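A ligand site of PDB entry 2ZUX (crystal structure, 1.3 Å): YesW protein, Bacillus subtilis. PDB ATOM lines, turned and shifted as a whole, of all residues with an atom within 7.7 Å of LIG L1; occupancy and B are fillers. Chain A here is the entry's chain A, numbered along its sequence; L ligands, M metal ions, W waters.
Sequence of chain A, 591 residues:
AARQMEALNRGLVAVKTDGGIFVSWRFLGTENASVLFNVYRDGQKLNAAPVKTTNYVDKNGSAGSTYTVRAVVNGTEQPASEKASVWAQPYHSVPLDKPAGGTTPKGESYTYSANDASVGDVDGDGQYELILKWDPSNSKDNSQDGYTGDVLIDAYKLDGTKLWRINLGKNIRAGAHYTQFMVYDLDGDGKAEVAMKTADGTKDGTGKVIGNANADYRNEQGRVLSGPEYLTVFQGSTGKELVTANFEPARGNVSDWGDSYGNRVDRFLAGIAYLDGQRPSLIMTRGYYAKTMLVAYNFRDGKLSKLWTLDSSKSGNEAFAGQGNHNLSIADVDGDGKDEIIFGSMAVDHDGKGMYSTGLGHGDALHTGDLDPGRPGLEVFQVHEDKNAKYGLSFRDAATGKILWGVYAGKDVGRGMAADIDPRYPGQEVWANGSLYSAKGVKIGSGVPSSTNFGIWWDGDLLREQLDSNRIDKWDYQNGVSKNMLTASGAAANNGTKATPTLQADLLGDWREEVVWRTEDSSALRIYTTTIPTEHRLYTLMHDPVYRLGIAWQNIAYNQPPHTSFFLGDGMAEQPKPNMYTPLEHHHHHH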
ATOM      1  N   ASN A 115      -5.942 -21.799  -9.267  1.00  0.00           N
ATOM      2  CA  ASN A 115      -5.108 -21.654  -8.084  1.00  0.00           C
ATOM      3  C   ASN A 115      -4.903 -23.042  -7.451  1.00  0.00           C
ATOM      4  O   ASN A 115      -4.666 -24.013  -8.182  1.00  0.00           O
ATOM      5  CB  ASN A 115      -5.731 -20.595  -7.162  1.00  0.00           C
ATOM      6  CG  ASN A 115      -4.756 -20.034  -6.137  1.00  0.00           C
ATOM      7  OD1 ASN A 115      -3.975 -19.096  -6.429  1.00  0.00           O
ATOM      8  ND2 ASN A 115      -4.833 -20.542  -4.932  1.00  0.00           N
ATOM      9  N   ASP A 135      -9.055 -18.212  -8.155  1.00  0.00           N
ATOM     10  CA  ASP A 135      -8.733 -17.031  -7.361  1.00  0.00           C
ATOM     11  C   ASP A 135      -9.011 -15.772  -8.173  1.00  0.00           C
ATOM     12  O   ASP A 135      -8.505 -15.620  -9.286  1.00  0.00           O
ATOM     13  CB  ASP A 135      -7.269 -17.045  -6.940  1.00  0.00           C
ATOM     14  CG  ASP A 135      -6.981 -16.084  -5.804  1.00  0.00           C
ATOM     15  OD1 ASP A 135      -7.648 -16.183  -4.753  1.00  0.00           O
ATOM     16  OD2 ASP A 135      -6.071 -15.249  -5.969  1.00  0.00           O
ATOM     17  N   SER A 139      -7.965 -10.921  -4.797  1.00  0.00           N
ATOM     18  CA  SER A 139      -7.920 -11.651  -3.534  1.00  0.00           C
ATOM     19  C   SER A 139      -6.962 -10.946  -2.567  1.00  0.00           C
ATOM     20  O   SER A 139      -6.052 -10.231  -2.982  1.00  0.00           O
ATOM     21  CB  SER A 139      -7.510 -13.098  -3.757  1.00  0.00           C
ATOM     22  OG  SER A 139      -6.216 -13.202  -4.307  1.00  0.00           O
ATOM     23  N   LYS A 140      -7.198 -11.142  -1.272  1.00  0.00           N
ATOM     24  CA  LYS A 140      -6.569 -10.299  -0.247  1.00  0.00           C
ATOM     25  C   LYS A 140      -5.889 -11.087   0.849  1.00  0.00           C
ATOM     26  O   LYS A 140      -6.418 -12.099   1.335  1.00  0.00           O
ATOM     27  CB  LYS A 140      -7.626  -9.411   0.404  1.00  0.00           C
ATOM     28  CG  LYS A 140      -8.218  -8.328  -0.508  1.00  0.00           C
ATOM     29  CD  LYS A 140      -7.245  -7.160  -0.672  1.00  0.00           C
ATOM     30  CE  LYS A 140      -7.746  -6.143  -1.708  1.00  0.00           C
ATOM     31  NZ  LYS A 140      -7.540  -6.646  -3.094  1.00  0.00           N
ATOM     32  N   ASP A 141      -4.714 -10.597   1.257  1.00  0.00           N
ATOM     33  CA  ASP A 141      -4.158 -10.999   2.537  1.00  0.00           C
ATOM     34  C   ASP A 141      -5.003 -10.410   3.662  1.00  0.00           C
ATOM     35  O   ASP A 141      -5.662  -9.378   3.483  1.00  0.00           O
ATOM     36  CB  ASP A 141      -2.714 -10.522   2.684  1.00  0.00           C
ATOM     37  CG  ASP A 141      -2.094 -10.977   3.990  1.00  0.00           C
ATOM     38  OD1 ASP A 141      -1.890 -12.197   4.131  1.00  0.00           O
ATOM     39  OD2 ASP A 141      -1.839 -10.125   4.863  1.00  0.00           O
ATOM     40  N   GLN A 144      -4.863  -6.701   4.472  1.00  0.00           N
ATOM     41  CA  GLN A 144      -5.314  -5.733   3.459  1.00  0.00           C
ATOM     42  C   GLN A 144      -6.823  -5.538   3.480  1.00  0.00           C
ATOM     43  O   GLN A 144      -7.576  -6.505   3.552  1.00  0.00           O
ATOM     44  CB  GLN A 144      -4.924  -6.216   2.072  1.00  0.00           C
ATOM     45  CG  GLN A 144      -3.451  -6.388   1.856  1.00  0.00           C
ATOM     46  CD  GLN A 144      -3.166  -6.992   0.505  1.00  0.00           C
ATOM     47  OE1 GLN A 144      -3.513  -8.142   0.233  1.00  0.00           O
ATOM     48  NE2 GLN A 144      -2.546  -6.205  -0.371  1.00  0.00           N
ATOM     49  N   GLY A 175      -8.788 -15.116  -0.523  1.00  0.00           N
ATOM     50  CA  GLY A 175      -7.404 -14.911  -0.101  1.00  0.00           C
ATOM     51  C   GLY A 175      -6.860 -16.208   0.467  1.00  0.00           C
ATOM     52  O   GLY A 175      -7.624 -17.116   0.797  1.00  0.00           O
ATOM     53  N   ALA A 176      -5.543 -16.286   0.595  1.00  0.00           N
ATOM     54  CA  ALA A 176      -4.875 -17.538   0.985  1.00  0.00           C
ATOM     55  C   ALA A 176      -5.376 -18.111   2.308  1.00  0.00           C
ATOM     56  O   ALA A 176      -5.407 -19.335   2.479  1.00  0.00           O
ATOM     57  CB  ALA A 176      -3.376 -17.325   1.030  1.00  0.00           C
ATOM     58  N   HIS A 177      -5.733 -17.234   3.245  1.00  0.00           N
ATOM     59  CA  HIS A 177      -5.983 -17.655   4.613  1.00  0.00           C
ATOM     60  C   HIS A 177      -7.440 -17.879   4.928  1.00  0.00           C
ATOM     61  O   HIS A 177      -7.770 -18.245   6.054  1.00  0.00           O
ATOM     62  CB  HIS A 177      -5.331 -16.664   5.568  1.00  0.00           C
ATOM     63  CG  HIS A 177      -3.878 -16.504   5.306  1.00  0.00           C
ATOM     64  ND1 HIS A 177      -2.970 -17.513   5.542  1.00  0.00           N
ATOM     65  CD2 HIS A 177      -3.193 -15.511   4.696  1.00  0.00           C
ATOM     66  CE1 HIS A 177      -1.774 -17.125   5.150  1.00  0.00           C
ATOM     67  NE2 HIS A 177      -1.889 -15.910   4.630  1.00  0.00           N
ATOM     68  N   ASP A 364       6.396 -19.783   8.923  1.00  0.00           N
ATOM     69  CA  ASP A 364       5.824 -19.827   7.580  1.00  0.00           C
ATOM     70  C   ASP A 364       6.024 -21.132   6.831  1.00  0.00           C
ATOM     71  O   ASP A 364       5.405 -21.330   5.787  1.00  0.00           O
ATOM     72  CB  ASP A 364       6.362 -18.677   6.724  1.00  0.00           C
ATOM     73  CG  ASP A 364       5.627 -17.386   6.952  1.00  0.00           C
ATOM     74  OD1 ASP A 364       5.211 -17.136   8.100  1.00  0.00           O
ATOM     75  OD2 ASP A 364       5.507 -16.591   5.978  1.00  0.00           O
ATOM     76  N   ARG A 415      11.333 -19.055   5.067  1.00  0.00           N
ATOM     77  CA  ARG A 415      11.307 -20.303   4.302  1.00  0.00           C
ATOM     78  C   ARG A 415      12.235 -21.320   4.953  1.00  0.00           C
ATOM     79  O   ARG A 415      13.273 -20.977   5.495  1.00  0.00           O
ATOM     80  CB  ARG A 415      11.772 -20.063   2.859  1.00  0.00           C
ATOM     81  CG  ARG A 415      10.959 -19.071   2.059  1.00  0.00           C
ATOM     82  CD  ARG A 415       9.552 -19.598   1.778  1.00  0.00           C
ATOM     83  NE  ARG A 415       8.914 -18.775   0.757  1.00  0.00           N
ATOM     84  CZ  ARG A 415       8.954 -19.026  -0.544  1.00  0.00           C
ATOM     85  NH1 ARG A 415       9.574 -20.096  -1.013  1.00  0.00           N
ATOM     86  NH2 ARG A 415       8.356 -18.190  -1.385  1.00  0.00           N
ATOM     87  N   ASN A 494       1.561 -20.431  -8.891  1.00  0.00           N
ATOM     88  CA  ASN A 494       0.519 -19.599  -8.285  1.00  0.00           C
ATOM     89  C   ASN A 494       1.008 -18.883  -7.027  1.00  0.00           C
ATOM     90  O   ASN A 494       2.092 -19.167  -6.509  1.00  0.00           O
ATOM     91  CB  ASN A 494      -0.708 -20.460  -7.869  1.00  0.00           C
ATOM     92  CG  ASN A 494      -1.173 -21.414  -8.946  1.00  0.00           C
ATOM     93  OD1 ASN A 494      -1.619 -22.529  -8.644  1.00  0.00           O
ATOM     94  ND2 ASN A 494      -1.094 -21.003 -10.190  1.00  0.00           N
ATOM     95  N   ASN A 495       0.174 -17.979  -6.531  1.00  0.00           N
ATOM     96  CA  ASN A 495       0.345 -17.382  -5.209  1.00  0.00           C
ATOM     97  C   ASN A 495       1.550 -16.464  -5.082  1.00  0.00           C
ATOM     98  O   ASN A 495       2.228 -16.444  -4.059  1.00  0.00           O
ATOM     99  CB  ASN A 495       0.298 -18.456  -4.094  1.00  0.00           C
ATOM    100  CG  ASN A 495      -1.001 -19.241  -4.106  1.00  0.00           C
ATOM    101  OD1 ASN A 495      -0.998 -20.489  -4.005  1.00  0.00           O
ATOM    102  ND2 ASN A 495      -2.104 -18.542  -4.221  1.00  0.00           N
ATOM    103  N   GLY A 496       1.787 -15.692  -6.138  1.00  0.00           N
ATOM    104  CA  GLY A 496       2.783 -14.634  -6.083  1.00  0.00           C
ATOM    105  C   GLY A 496       4.148 -15.172  -5.713  1.00  0.00           C
ATOM    106  O   GLY A 496       4.644 -16.105  -6.323  1.00  0.00           O
ATOM    107  N   THR A 497       4.745 -14.584  -4.690  1.00  0.00           N
ATOM    108  CA  THR A 497       6.096 -14.974  -4.304  1.00  0.00           C
ATOM    109  C   THR A 497       6.171 -16.412  -3.781  1.00  0.00           C
ATOM    110  O   THR A 497       7.251 -17.010  -3.763  1.00  0.00           O
ATOM    111  CB  THR A 497       6.696 -14.027  -3.243  1.00  0.00           C
ATOM    112  OG1 THR A 497       5.914 -14.081  -2.047  1.00  0.00           O
ATOM    113  CG2 THR A 497       6.741 -12.586  -3.769  1.00  0.00           C
ATOM    114  N   LYS A 498       5.041 -16.980  -3.364  1.00  0.00           N
ATOM    115  CA  LYS A 498       5.044 -18.373  -2.915  1.00  0.00           C
ATOM    116  C   LYS A 498       5.329 -19.340  -4.068  1.00  0.00           C
ATOM    117  O   LYS A 498       5.930 -20.398  -3.849  1.00  0.00           O
ATOM    118  CB  LYS A 498       3.737 -18.735  -2.211  1.00  0.00           C
ATOM    119  CG  LYS A 498       3.454 -17.895  -0.970  1.00  0.00           C
ATOM    120  CD  LYS A 498       4.476 -18.128   0.154  1.00  0.00           C
ATOM    121  CE  LYS A 498       4.237 -17.182   1.306  1.00  0.00           C
ATOM    122  NZ  LYS A 498       5.243 -17.391   2.386  1.00  0.00           N
ATOM    123  N   ALA A 499       4.925 -18.968  -5.284  1.00  0.00           N
ATOM    124  CA  ALA A 499       5.271 -19.709  -6.515  1.00  0.00           C
ATOM    125  C   ALA A 499       5.019 -21.219  -6.385  1.00  0.00           C
ATOM    126  O   ALA A 499       5.921 -22.043  -6.616  1.00  0.00           O
ATOM    127  CB  ALA A 499       6.719 -19.409  -6.921  1.00  0.00           C
ATOM    128  N   THR A 500       3.790 -21.560  -6.028  1.00  0.00           N
ATOM    129  CA  THR A 500       3.404 -22.949  -5.786  1.00  0.00           C
ATOM    130  C   THR A 500       2.698 -23.561  -6.999  1.00  0.00           C
ATOM    131  O   THR A 500       1.991 -22.865  -7.720  1.00  0.00           O
ATOM    132  CB  THR A 500       2.468 -23.058  -4.559  1.00  0.00           C
ATOM    133  OG1 THR A 500       1.341 -22.182  -4.727  1.00  0.00           O
ATOM    134  CG2 THR A 500       3.225 -22.683  -3.285  1.00  0.00           C
ATOM    135  N   ALA A 557      -3.658 -22.480   3.236  1.00  0.00           N
ATOM    136  CA  ALA A 557      -2.877 -21.271   3.495  1.00  0.00           C
ATOM    137  C   ALA A 557      -1.577 -21.293   2.681  1.00  0.00           C
ATOM    138  O   ALA A 557      -1.638 -21.334   1.441  1.00  0.00           O
ATOM    139  CB  ALA A 557      -2.646 -21.078   4.998  1.00  0.00           C
ATOM    140  N   TYR A 558      -0.412 -21.244   3.315  1.00  0.00           N
ATOM    141  CA  TYR A 558       0.840 -21.300   2.559  1.00  0.00           C
ATOM    142  C   TYR A 558       1.274 -22.733   2.299  1.00  0.00           C
ATOM    143  O   TYR A 558       1.942 -23.358   3.113  1.00  0.00           O
ATOM    144  CB  TYR A 558       1.944 -20.477   3.234  1.00  0.00           C
ATOM    145  CG  TYR A 558       1.673 -18.979   3.283  1.00  0.00           C
ATOM    146  CD1 TYR A 558       0.701 -18.379   2.473  1.00  0.00           C
ATOM    147  CD2 TYR A 558       2.390 -18.160   4.139  1.00  0.00           C
ATOM    148  CE1 TYR A 558       0.483 -16.989   2.521  1.00  0.00           C
ATOM    149  CE2 TYR A 558       2.167 -16.782   4.199  1.00  0.00           C
ATOM    150  CZ  TYR A 558       1.202 -16.213   3.384  1.00  0.00           C
ATOM    151  OH  TYR A 558       0.940 -14.860   3.409  1.00  0.00           O
ATOM    152  N   ASN A 559       0.869 -23.203   1.119  1.00  0.00           N
ATOM    153  CA  ASN A 559       1.044 -24.599   0.693  1.00  0.00           C
ATOM    154  C   ASN A 559       2.442 -25.102   1.017  1.00  0.00           C
ATOM    155  O   ASN A 559       3.429 -24.459   0.649  1.00  0.00           O
ATOM    156  CB  ASN A 559       0.900 -24.733  -0.832  1.00  0.00           C
ATOM    157  CG  ASN A 559      -0.375 -24.119  -1.396  1.00  0.00           C
ATOM    158  OD1 ASN A 559      -0.914 -23.130  -0.888  1.00  0.00           O
ATOM    159  ND2 ASN A 559      -0.813 -24.655  -2.530  1.00  0.00           N
HETATM  160  C1  LIG L   1      -0.209 -14.688  -1.046  1.00  0.00           C
HETATM  161  C2  LIG L   1       1.150 -14.627  -0.347  1.00  0.00           C
HETATM  162  C3  LIG L   1       2.264 -14.299  -1.341  1.00  0.00           C
HETATM  163  C4  LIG L   1       1.941 -13.041  -2.148  1.00  0.00           C
HETATM  164  C5  LIG L   1       0.557 -13.184  -2.787  1.00  0.00           C
HETATM  165  C6  LIG L   1       0.158 -11.893  -3.479  1.00  0.00           C
HETATM  166  O1  LIG L   1      -0.296 -15.852  -1.838  1.00  0.00           O
HETATM  167  O2  LIG L   1       1.065 -13.640   0.655  1.00  0.00           O
HETATM  168  O3  LIG L   1       3.498 -14.138  -0.672  1.00  0.00           O
HETATM  169  O4  LIG L   1       2.948 -12.811  -3.109  1.00  0.00           O
HETATM  170  O5  LIG L   1      -0.435 -13.523  -1.827  1.00  0.00           O
HETATM  171  C1  LG2 L   2      -1.161 -13.242  -6.634  1.00  0.00           C
HETATM  172  C2  LG2 L   2      -2.393 -14.085  -6.245  1.00  0.00           C
HETATM  173  C3  LG2 L   2      -2.756 -15.156  -7.285  1.00  0.00           C
HETATM  174  C4  LG2 L   2      -1.499 -15.852  -7.791  1.00  0.00           C
HETATM  175  C5  LG2 L   2      -0.614 -14.803  -8.436  1.00  0.00           C
HETATM  176  C6  LG2 L   2       0.637 -15.420  -9.046  1.00  0.00           C
HETATM  177  O1  LG2 L   2      -1.586 -12.048  -7.247  1.00  0.00           O
HETATM  178  O2  LG2 L   2      -2.143 -14.701  -4.997  1.00  0.00           O
HETATM  179  O3  LG2 L   2      -3.675 -16.075  -6.755  1.00  0.00           O
HETATM  180  O4  LG2 L   2      -1.764 -16.947  -8.652  1.00  0.00           O
HETATM  181  O5  LG2 L   2      -0.186 -13.873  -7.445  1.00  0.00           O
HETATM  182 CA    CA M   1      -3.004 -22.059  -0.374  1.00  0.00          CA
HETATM  183  O   HOH W   1      -0.104 -10.928   0.163  1.00  0.00           O
HETATM  184  O   HOH W   2      -1.559 -13.881   2.084  1.00  0.00           O
HETATM  185  O   HOH W   3      -2.774 -16.380  -2.606  1.00  0.00           O
HETATM  186  O   HOH W   4       3.584 -10.195  -3.085  1.00  0.00           O
HETATM  187  O   HOH W   5      -0.479 -18.367  -0.644  1.00  0.00           O
HETATM  188  O   HOH W   6      -2.897 -12.418  -1.394  1.00  0.00           O
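Gly 496 touches LIG L1 (CA to O4, 3.5 Å). CE of Lys 498 touches O3 of LIG L1, at 3.7 Å. Hydrophobic or aromatic side chains that line LIG L1: Tyr 558. Five residues have an atom within 4 Å of LIG L1: Asn 495, Gly 496, Thr 497, Lys 498 and Tyr 558.
Water W3 lies within hydrogen-bond range of O1 of LIG L1 (2.6 Å), ND2 of Asn 495 (2.8 Å) and O2 of LG2 L2 (3.0 Å). Water W2 lies within hydrogen-bond range of OD1 of Asp 141, OH of Tyr 558, O2 of LIG L1 and NE2 of His 177.
O of Thr 497 is in hydrogen-bond range of NH2 of Arg 415, at 2.9 Å. The side-chain hydroxyl (OH) of Tyr 558 sits at hydrogen-bond distance from a ring nitrogen (NE2) of His 177 (3.3 Å). ND2 of Asn 495 lies within hydrogen-bond range of OD1 of Asn 115, 2.9 Å away. The side-chain hydroxyl (OG1) of Thr 500 is in hydrogen-bond range of the side-chain amide oxygen (OD1) of Asn 495 (3.0 Å). The side-chain amino group of Lys 498 lies within salt-bridge range of the side-chain carboxylate of Asp 364, at 3.7 Å.
The backbone NH of Thr 497 is in hydrogen-bond range of an oxygen (O4) of LIG L1. O3 of LIG L1 lies within hydrogen-bond range of OG1 of Thr 497, at 2.8 Å. OH of Tyr 558 sits at hydrogen-bond distance from O2 of LIG L1. The backbone carbonyl oxygen (O) of Asn 495 lies within hydrogen-bond range of an oxygen (O1) of LIG L1, 3.4 Å away. The backbone NH (N) of Asn 495 sits close to an oxygen (O4) of LG2 L2, 3.1 Å away. The backbone NH (N) of Gly 496 is in hydrogen-bond range of an oxygen (O5) of LG2 L2 (3.0 Å). The side-chain amide oxygen (OD1) of Asn 115 sits at hydrogen-bond distance from an oxygen (O3) of LG2 L2 (3.1 Å). O3 of LG2 L2 lies within hydrogen-bond range of OD2 of Asp 135 (2.7 Å).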
